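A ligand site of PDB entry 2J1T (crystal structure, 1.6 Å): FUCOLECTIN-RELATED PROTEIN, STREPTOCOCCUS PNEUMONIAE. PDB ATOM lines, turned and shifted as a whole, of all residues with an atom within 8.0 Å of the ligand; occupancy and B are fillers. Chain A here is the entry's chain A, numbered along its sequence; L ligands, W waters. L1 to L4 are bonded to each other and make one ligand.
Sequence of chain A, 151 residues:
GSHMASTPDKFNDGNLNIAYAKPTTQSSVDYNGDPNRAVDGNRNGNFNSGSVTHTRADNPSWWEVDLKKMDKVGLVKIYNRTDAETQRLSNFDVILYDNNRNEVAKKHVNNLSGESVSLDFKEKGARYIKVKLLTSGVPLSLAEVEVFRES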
ATOM      1  N   ASP A  30      -3.432   2.097 -10.486  1.00  0.00           N
ATOM      2  CA  ASP A  30      -4.051   1.735  -9.210  1.00  0.00           C
ATOM      3  C   ASP A  30      -3.655   0.302  -8.883  1.00  0.00           C
ATOM      4  O   ASP A  30      -3.346  -0.508  -9.779  1.00  0.00           O
ATOM      5  CB  ASP A  30      -5.585   1.966  -9.276  1.00  0.00           C
ATOM      6  CG  ASP A  30      -6.192   2.243  -7.905  1.00  0.00           C
ATOM      7  OD1 ASP A  30      -5.423   2.324  -6.888  1.00  0.00           O
ATOM      8  OD2 ASP A  30      -7.413   2.473  -7.794  1.00  0.00           O
ATOM      9  N   TYR A  31      -3.600  -0.028  -7.594  1.00  0.00           N
ATOM     10  CA  TYR A  31      -3.320  -1.371  -7.110  1.00  0.00           C
ATOM     11  C   TYR A  31      -1.993  -1.927  -7.622  1.00  0.00           C
ATOM     12  O   TYR A  31      -1.867  -3.119  -7.817  1.00  0.00           O
ATOM     13  CB  TYR A  31      -4.452  -2.342  -7.404  1.00  0.00           C
ATOM     14  CG  TYR A  31      -5.801  -1.917  -6.820  1.00  0.00           C
ATOM     15  CD1 TYR A  31      -6.763  -1.364  -7.627  1.00  0.00           C
ATOM     16  CD2 TYR A  31      -6.081  -2.070  -5.472  1.00  0.00           C
ATOM     17  CE1 TYR A  31      -8.002  -0.963  -7.130  1.00  0.00           C
ATOM     18  CE2 TYR A  31      -7.303  -1.690  -4.956  1.00  0.00           C
ATOM     19  CZ  TYR A  31      -8.267  -1.141  -5.813  1.00  0.00           C
ATOM     20  OH  TYR A  31      -9.498  -0.724  -5.321  1.00  0.00           O
ATOM     21  N   ASN A  32      -1.047  -1.016  -7.893  1.00  0.00           N
ATOM     22  CA  ASN A  32       0.281  -1.352  -8.415  1.00  0.00           C
ATOM     23  C   ASN A  32       0.212  -2.023  -9.766  1.00  0.00           C
ATOM     24  O   ASN A  32       1.195  -2.675 -10.199  1.00  0.00           O
ATOM     25  CB  ASN A  32       1.072  -2.194  -7.397  1.00  0.00           C
ATOM     26  CG  ASN A  32       1.233  -1.507  -6.078  1.00  0.00           C
ATOM     27  OD1 ASN A  32       1.483  -0.320  -6.043  1.00  0.00           O
ATOM     28  ND2 ASN A  32       1.117  -2.267  -4.993  1.00  0.00           N
ATOM     29  N   ASN A  46      -5.216 -13.493 -13.785  1.00  0.00           N
ATOM     30  CA  ASN A  46      -5.585 -13.319 -12.379  1.00  0.00           C
ATOM     31  C   ASN A  46      -4.853 -12.105 -11.851  1.00  0.00           C
ATOM     32  O   ASN A  46      -3.640 -12.054 -11.821  1.00  0.00           O
ATOM     33  CB  ASN A  46      -5.336 -14.593 -11.574  1.00  0.00           C
ATOM     34  CG  ASN A  46      -5.869 -14.516 -10.212  1.00  0.00           C
ATOM     35  OD1 ASN A  46      -5.940 -13.419  -9.604  1.00  0.00           O
ATOM     36  ND2 ASN A  46      -6.236 -15.698  -9.641  1.00  0.00           N
ATOM     37  N   PHE A  47      -5.613 -11.092 -11.448  1.00  0.00           N
ATOM     38  CA  PHE A  47      -5.000  -9.862 -11.022  1.00  0.00           C
ATOM     39  C   PHE A  47      -4.003 -10.103  -9.893  1.00  0.00           C
ATOM     40  O   PHE A  47      -2.966  -9.451  -9.805  1.00  0.00           O
ATOM     41  CB  PHE A  47      -6.051  -8.799 -10.589  1.00  0.00           C
ATOM     42  CG  PHE A  47      -5.420  -7.493 -10.285  1.00  0.00           C
ATOM     43  CD1 PHE A  47      -5.169  -7.125  -8.996  1.00  0.00           C
ATOM     44  CD2 PHE A  47      -4.940  -6.674 -11.319  1.00  0.00           C
ATOM     45  CE1 PHE A  47      -4.494  -5.946  -8.722  1.00  0.00           C
ATOM     46  CE2 PHE A  47      -4.242  -5.505 -11.005  1.00  0.00           C
ATOM     47  CZ  PHE A  47      -4.014  -5.161  -9.701  1.00  0.00           C
ATOM     48  N   ASN A  48      -4.290 -11.068  -9.046  1.00  0.00           N
ATOM     49  CA  ASN A  48      -3.379 -11.317  -7.917  1.00  0.00           C
ATOM     50  C   ASN A  48      -2.047 -11.979  -8.247  1.00  0.00           C
ATOM     51  O   ASN A  48      -1.133 -12.023  -7.361  1.00  0.00           O
ATOM     52  CB  ASN A  48      -4.105 -12.020  -6.810  1.00  0.00           C
ATOM     53  CG  ASN A  48      -5.080 -11.102  -6.105  1.00  0.00           C
ATOM     54  OD1 ASN A  48      -4.834  -9.856  -5.939  1.00  0.00           O
ATOM     55  ND2 ASN A  48      -6.198 -11.660  -5.706  1.00  0.00           N
ATOM     56  N   THR A  53      -2.464  -5.288 -15.638  1.00  0.00           N
ATOM     57  CA  THR A  53      -2.446  -3.850 -15.388  1.00  0.00           C
ATOM     58  C   THR A  53      -3.716  -3.412 -14.686  1.00  0.00           C
ATOM     59  O   THR A  53      -4.670  -4.164 -14.576  1.00  0.00           O
ATOM     60  CB  THR A  53      -2.302  -3.081 -16.685  1.00  0.00           C
ATOM     61  OG1 THR A  53      -3.511  -3.202 -17.459  1.00  0.00           O
ATOM     62  CG2 THR A  53      -1.113  -3.588 -17.576  1.00  0.00           C
ATOM     63  N   HIS A  54      -3.708  -2.161 -14.243  1.00  0.00           N
ATOM     64  CA  HIS A  54      -4.876  -1.536 -13.598  1.00  0.00           C
ATOM     65  C   HIS A  54      -4.687  -0.033 -13.526  1.00  0.00           C
ATOM     66  O   HIS A  54      -3.744   0.491 -12.925  1.00  0.00           O
ATOM     67  CB  HIS A  54      -5.009  -2.082 -12.194  1.00  0.00           C
ATOM     68  CG  HIS A  54      -6.401  -2.075 -11.639  1.00  0.00           C
ATOM     69  ND1 HIS A  54      -7.105  -0.918 -11.343  1.00  0.00           N
ATOM     70  CD2 HIS A  54      -7.170  -3.110 -11.219  1.00  0.00           C
ATOM     71  CE1 HIS A  54      -8.268  -1.248 -10.813  1.00  0.00           C
ATOM     72  NE2 HIS A  54      -8.336  -2.572 -10.710  1.00  0.00           N
ATOM     73  N   THR A  55      -5.599   0.678 -14.147  1.00  0.00           N
ATOM     74  CA  THR A  55      -5.612   2.155 -13.996  1.00  0.00           C
ATOM     75  C   THR A  55      -6.621   2.541 -12.906  1.00  0.00           C
ATOM     76  O   THR A  55      -7.383   1.702 -12.422  1.00  0.00           O
ATOM     77  CB  THR A  55      -6.015   2.871 -15.322  1.00  0.00           C
ATOM     78  OG1 THR A  55      -7.403   2.579 -15.624  1.00  0.00           O
ATOM     79  CG2 THR A  55      -5.277   2.370 -16.532  1.00  0.00           C
ATOM     80  N   ARG A  81      -8.236  -9.437 -18.067  1.00  0.00           N
ATOM     81  CA  ARG A  81      -8.402  -9.910 -16.720  1.00  0.00           C
ATOM     82  C   ARG A  81      -9.430 -11.081 -16.697  1.00  0.00           C
ATOM     83  O   ARG A  81     -10.399 -11.080 -17.432  1.00  0.00           O
ATOM     84  CB  ARG A  81      -8.869  -8.745 -15.809  1.00  0.00           C
ATOM     85  CG  ARG A  81      -8.796  -9.078 -14.312  1.00  0.00           C
ATOM     86  CD  ARG A  81      -9.216  -8.003 -13.396  1.00  0.00           C
ATOM     87  NE  ARG A  81      -9.252  -8.455 -12.019  1.00  0.00           N
ATOM     88  CZ  ARG A  81      -9.584  -7.704 -11.013  1.00  0.00           C
ATOM     89  NH1 ARG A  81      -9.924  -6.465 -11.201  1.00  0.00           N
ATOM     90  NH2 ARG A  81      -9.580  -8.179  -9.772  1.00  0.00           N
ATOM     91  N   ASP A  83      -9.951 -13.094 -13.316  1.00  0.00           N
ATOM     92  CA  ASP A  83     -10.419 -13.496 -11.969  1.00  0.00           C
ATOM     93  C   ASP A  83     -11.674 -12.754 -11.535  1.00  0.00           C
ATOM     94  O   ASP A  83     -12.475 -13.289 -10.707  1.00  0.00           O
ATOM     95  CB  ASP A  83      -9.374 -13.287 -10.888  1.00  0.00           C
ATOM     96  CG  ASP A  83      -9.009 -11.822 -10.702  1.00  0.00           C
ATOM     97  OD1 ASP A  83      -9.278 -11.229  -9.620  1.00  0.00           O
ATOM     98  OD2 ASP A  83      -8.485 -11.193 -11.641  1.00  0.00           O
ATOM     99  N   ALA A  84     -11.837 -11.511 -11.993  1.00  0.00           N
ATOM    100  CA  ALA A  84     -12.985 -10.686 -11.605  1.00  0.00           C
ATOM    101  C   ALA A  84     -13.157  -9.544 -12.625  1.00  0.00           C
ATOM    102  O   ALA A  84     -12.243  -9.227 -13.353  1.00  0.00           O
ATOM    103  CB  ALA A  84     -12.794 -10.104 -10.247  1.00  0.00           C
ATOM    104  N   GLU A  85     -14.322  -8.907 -12.600  1.00  0.00           N
ATOM    105  CA  GLU A  85     -14.574  -7.642 -13.298  1.00  0.00           C
ATOM    106  C   GLU A  85     -14.279  -7.745 -14.804  1.00  0.00           C
ATOM    107  O   GLU A  85     -13.812  -6.815 -15.412  1.00  0.00           O
ATOM    108  CB  GLU A  85     -13.813  -6.499 -12.653  1.00  0.00           C
ATOM    109  CG  GLU A  85     -14.073  -6.302 -11.157  1.00  0.00           C
ATOM    110  CD  GLU A  85     -15.441  -5.749 -10.820  1.00  0.00           C
ATOM    111  OE1 GLU A  85     -16.314  -5.595 -11.721  1.00  0.00           O
ATOM    112  OE2 GLU A  85     -15.659  -5.446  -9.620  1.00  0.00           O
ATOM    113  N   GLN A  87     -16.099  -7.765 -17.336  1.00  0.00           N
ATOM    114  CA  GLN A  87     -16.908  -6.947 -18.174  1.00  0.00           C
ATOM    115  C   GLN A  87     -16.315  -5.571 -18.410  1.00  0.00           C
ATOM    116  O   GLN A  87     -16.746  -4.860 -19.340  1.00  0.00           O
ATOM    117  CB  GLN A  87     -18.295  -6.782 -17.551  1.00  0.00           C
ATOM    118  CG  GLN A  87     -18.411  -5.799 -16.407  1.00  0.00           C
ATOM    119  CD  GLN A  87     -17.707  -6.197 -15.139  1.00  0.00           C
ATOM    120  OE1 GLN A  87     -17.526  -7.406 -14.871  1.00  0.00           O
ATOM    121  NE2 GLN A  87     -17.368  -5.228 -14.334  1.00  0.00           N
ATOM    122  N   ARG A  88     -15.310  -5.183 -17.607  1.00  0.00           N
ATOM    123  CA  ARG A  88     -14.739  -3.836 -17.765  1.00  0.00           C
ATOM    124  C   ARG A  88     -14.097  -3.708 -19.139  1.00  0.00           C
ATOM    125  O   ARG A  88     -14.093  -2.619 -19.706  1.00  0.00           O
ATOM    126  CB  ARG A  88     -13.689  -3.534 -16.714  1.00  0.00           C
ATOM    127  CG  ARG A  88     -14.313  -3.353 -15.334  1.00  0.00           C
ATOM    128  CD  ARG A  88     -13.241  -3.175 -14.252  1.00  0.00           C
ATOM    129  NE  ARG A  88     -13.885  -2.761 -13.005  1.00  0.00           N
ATOM    130  CZ  ARG A  88     -13.294  -2.767 -11.832  1.00  0.00           C
ATOM    131  NH1 ARG A  88     -12.004  -3.146 -11.714  1.00  0.00           N
ATOM    132  NH2 ARG A  88     -13.975  -2.386 -10.750  1.00  0.00           N
ATOM    133  N   PRO A 139     -11.979   1.340 -14.513  1.00  0.00           N
ATOM    134  CA  PRO A 139     -10.547   0.971 -14.651  1.00  0.00           C
ATOM    135  C   PRO A 139     -10.290   0.041 -15.849  1.00  0.00           C
ATOM    136  O   PRO A 139     -11.069  -0.849 -16.120  1.00  0.00           O
ATOM    137  CB  PRO A 139     -10.246   0.221 -13.376  1.00  0.00           C
ATOM    138  CG  PRO A 139     -11.356   0.651 -12.420  1.00  0.00           C
ATOM    139  CD  PRO A 139     -12.569   0.802 -13.272  1.00  0.00           C
ATOM    140  N   SER A 141      -7.871  -2.835 -17.156  1.00  0.00           N
ATOM    141  CA  SER A 141      -6.970  -3.888 -16.760  1.00  0.00           C
ATOM    142  C   SER A 141      -6.771  -4.854 -17.906  1.00  0.00           C
ATOM    143  O   SER A 141      -7.714  -5.431 -18.431  1.00  0.00           O
ATOM    144  CB  SER A 141      -7.535  -4.661 -15.580  1.00  0.00           C
ATOM    145  OG  SER A 141      -7.506  -3.916 -14.354  1.00  0.00           O
HETATM  146  C1  LIG L   1     -11.955  -6.142  -7.430  1.00  0.00           C
HETATM  147  C2  LIG L   1     -12.528  -4.862  -8.100  1.00  0.00           C
HETATM  148  C3  LIG L   1     -11.714  -3.601  -7.777  1.00  0.00           C
HETATM  149  C4  LIG L   1     -10.255  -3.866  -8.135  1.00  0.00           C
HETATM  150  C5  LIG L   1      -9.786  -5.116  -7.372  1.00  0.00           C
HETATM  151  C6  LIG L   1      -8.318  -5.396  -7.629  1.00  0.00           C
HETATM  152  O1  LIG L   1     -13.897  -4.629  -7.759  1.00  0.00           O
HETATM  153  O2  LIG L   1     -12.189  -2.496  -8.472  1.00  0.00           O
HETATM  154  O3  LIG L   1     -10.179  -4.118  -9.522  1.00  0.00           O
HETATM  155  O4  LIG L   1     -10.554  -6.309  -7.652  1.00  0.00           O
HETATM  156  C1  LG2 L   2     -11.486  -6.785  -3.881  1.00  0.00           C
HETATM  157  C2  LG2 L   2     -12.209  -7.070  -5.208  1.00  0.00           C
HETATM  158  C3  LG2 L   2     -13.657  -7.382  -4.906  1.00  0.00           C
HETATM  159  C4  LG2 L   2     -13.663  -8.506  -3.845  1.00  0.00           C
HETATM  160  C5  LG2 L   2     -12.831  -8.186  -2.609  1.00  0.00           C
HETATM  161  C6  LG2 L   2     -12.750  -9.307  -1.562  1.00  0.00           C
HETATM  162  O1  LG2 L   2     -12.165  -5.918  -6.042  1.00  0.00           O
HETATM  163  O2  LG2 L   2     -14.282  -7.876  -6.068  1.00  0.00           O
HETATM  164  O3  LG2 L   2     -13.127  -9.673  -4.441  1.00  0.00           O
HETATM  165  O4  LG2 L   2     -11.497  -7.910  -2.983  1.00  0.00           O
HETATM  166  O5  LG2 L   2     -12.201  -8.727  -0.401  1.00  0.00           O
HETATM  167  C1  LG3 L   3      -7.107  -4.466  -2.345  1.00  0.00           C
HETATM  168  C2  LG3 L   3      -7.223  -5.944  -2.020  1.00  0.00           C
HETATM  169  C3  LG3 L   3      -8.074  -6.598  -3.083  1.00  0.00           C
HETATM  170  C4  LG3 L   3      -9.406  -5.862  -3.192  1.00  0.00           C
HETATM  171  C5  LG3 L   3      -9.204  -4.356  -3.403  1.00  0.00           C
HETATM  172  C6  LG3 L   3     -10.486  -3.528  -3.389  1.00  0.00           C
HETATM  173  C7  LG3 L   3      -5.372  -6.924  -0.756  1.00  0.00           C
HETATM  174  C8  LG3 L   3      -3.892  -6.659  -0.725  1.00  0.00           C
HETATM  175  N1  LG3 L   3      -5.939  -6.617  -1.921  1.00  0.00           N
HETATM  176  O1  LG3 L   3      -6.412  -3.754  -1.367  1.00  0.00           O
HETATM  177  O2  LG3 L   3      -8.355  -7.913  -2.660  1.00  0.00           O
HETATM  178  O3  LG3 L   3     -10.153  -6.460  -4.211  1.00  0.00           O
HETATM  179  O4  LG3 L   3      -8.412  -3.935  -2.324  1.00  0.00           O
HETATM  180  O5  LG3 L   3     -11.106  -3.621  -2.116  1.00  0.00           O
HETATM  181  O6  LG3 L   3      -5.985  -7.393   0.212  1.00  0.00           O
HETATM  182  C1  LG4 L   4      -7.548  -9.165  -3.281  1.00  0.00           C
HETATM  183  C2  LG4 L   4      -7.885 -10.533  -2.697  1.00  0.00           C
HETATM  184  C3  LG4 L   4      -9.339 -10.874  -3.016  1.00  0.00           C
HETATM  185  C4  LG4 L   4      -9.574 -10.811  -4.524  1.00  0.00           C
HETATM  186  C5  LG4 L   4      -9.154  -9.441  -5.075  1.00  0.00           C
HETATM  187  C6  LG4 L   4      -9.196  -9.352  -6.593  1.00  0.00           C
HETATM  188  O1  LG4 L   4      -7.662 -10.320  -1.321  1.00  0.00           O
HETATM  189  O2  LG4 L   4      -9.735 -12.167  -2.557  1.00  0.00           O
HETATM  190  O3  LG4 L   4      -8.804 -11.853  -5.097  1.00  0.00           O
HETATM  191  O4  LG4 L   4      -7.851  -9.084  -4.649  1.00  0.00           O
HETATM  192  O   HOH W   1      -4.746  -6.072  -4.964  1.00  0.00           O
HETATM  193  O   HOH W   2     -14.765  -3.424  -5.450  1.00  0.00           O
HETATM  194  O   HOH W   3     -10.522 -12.522   0.025  1.00  0.00           O
HETATM  195  O   HOH W   4     -10.027 -12.537  -7.496  1.00  0.00           O
HETATM  196  O   HOH W   5     -14.271  -7.710   1.274  1.00  0.00           O
HETATM  197  O   HOH W   6     -12.742 -13.062  -4.156  1.00  0.00           O
HETATM  198  O   HOH W   7      -9.417  -8.396  -0.105  1.00  0.00           O
HETATM  199  O   HOH W   8     -14.775 -10.593  -7.025  1.00  0.00           O
HETATM  200  O   HOH W   9      -6.255  -9.601   2.654  1.00  0.00           O
HETATM  201  O   HOH W  10     -11.482  -0.117  -7.293  1.00  0.00           O
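Water W10 bridges O2 of LIG L1 and OH of Tyr 31.
Water W4 bridges the side-chain carboxylate (OD1) of Asp 83 and an oxygen (O3) of LG4 L4.
Tyr 31 touches the ligand.
CD1 of Phe 47 touches C6 of LIG L1, 3.8 Å away.
Asp 83 touches the ligand.
Within 4 Å of the ligand: Tyr 31, Phe 47, Asn 48, His 54, Arg 81, Asp 83, Glu 85 and Arg 88.
The nearest printed residue that does not touch the ligand is Ala 84 (4.9 Å).
The backbone carbonyl oxygen (O) of His 54 lies within hydrogen-bond range of the backbone NH (N) of Asp 30.
The side-chain amide oxygen of Asn 46 is in hydrogen-bond range of the backbone NH of Asn 48 (2.9 Å).
The backbone NH (N) of Phe 47 lies within hydrogen-bond range of the side-chain carboxylate (OD2) of Asp 83.
The side-chain carboxylate (OE2) of Glu 85 is in salt-bridge range of the guanidinium group (NH2) of Arg 88, at 3.7 Å.
NE of Arg 81 lies close to O of Ala 84 (3.4 Å).
The guanidinium group (NE) of Arg 81 lies within salt-bridge range of the side-chain carboxylate (OD2) of Asp 83 (2.9 Å).
The side-chain carboxylate (OE1) of Glu 85 is in hydrogen-bond range of the side-chain amide nitrogen (NE2) of Gln 87 (2.8 Å).
The side-chain carboxylate (OE2) of Glu 85 is in hydrogen-bond range of an oxygen (O1) of LIG L1.
The guanidinium group (NH1) of Arg 81 is in hydrogen-bond range of an oxygen (O3) of LIG L1, at 2.9 Å.
NE2 of His 54 is in hydrogen-bond range of O3 of LIG L1.
The guanidinium group of Arg 88 sits at hydrogen-bond distance from an oxygen (O2) of LIG L1 (2.9 Å).
ND2 of Asn 48 lies within hydrogen-bond range of O3 of LG4 L4 (2.7 Å).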
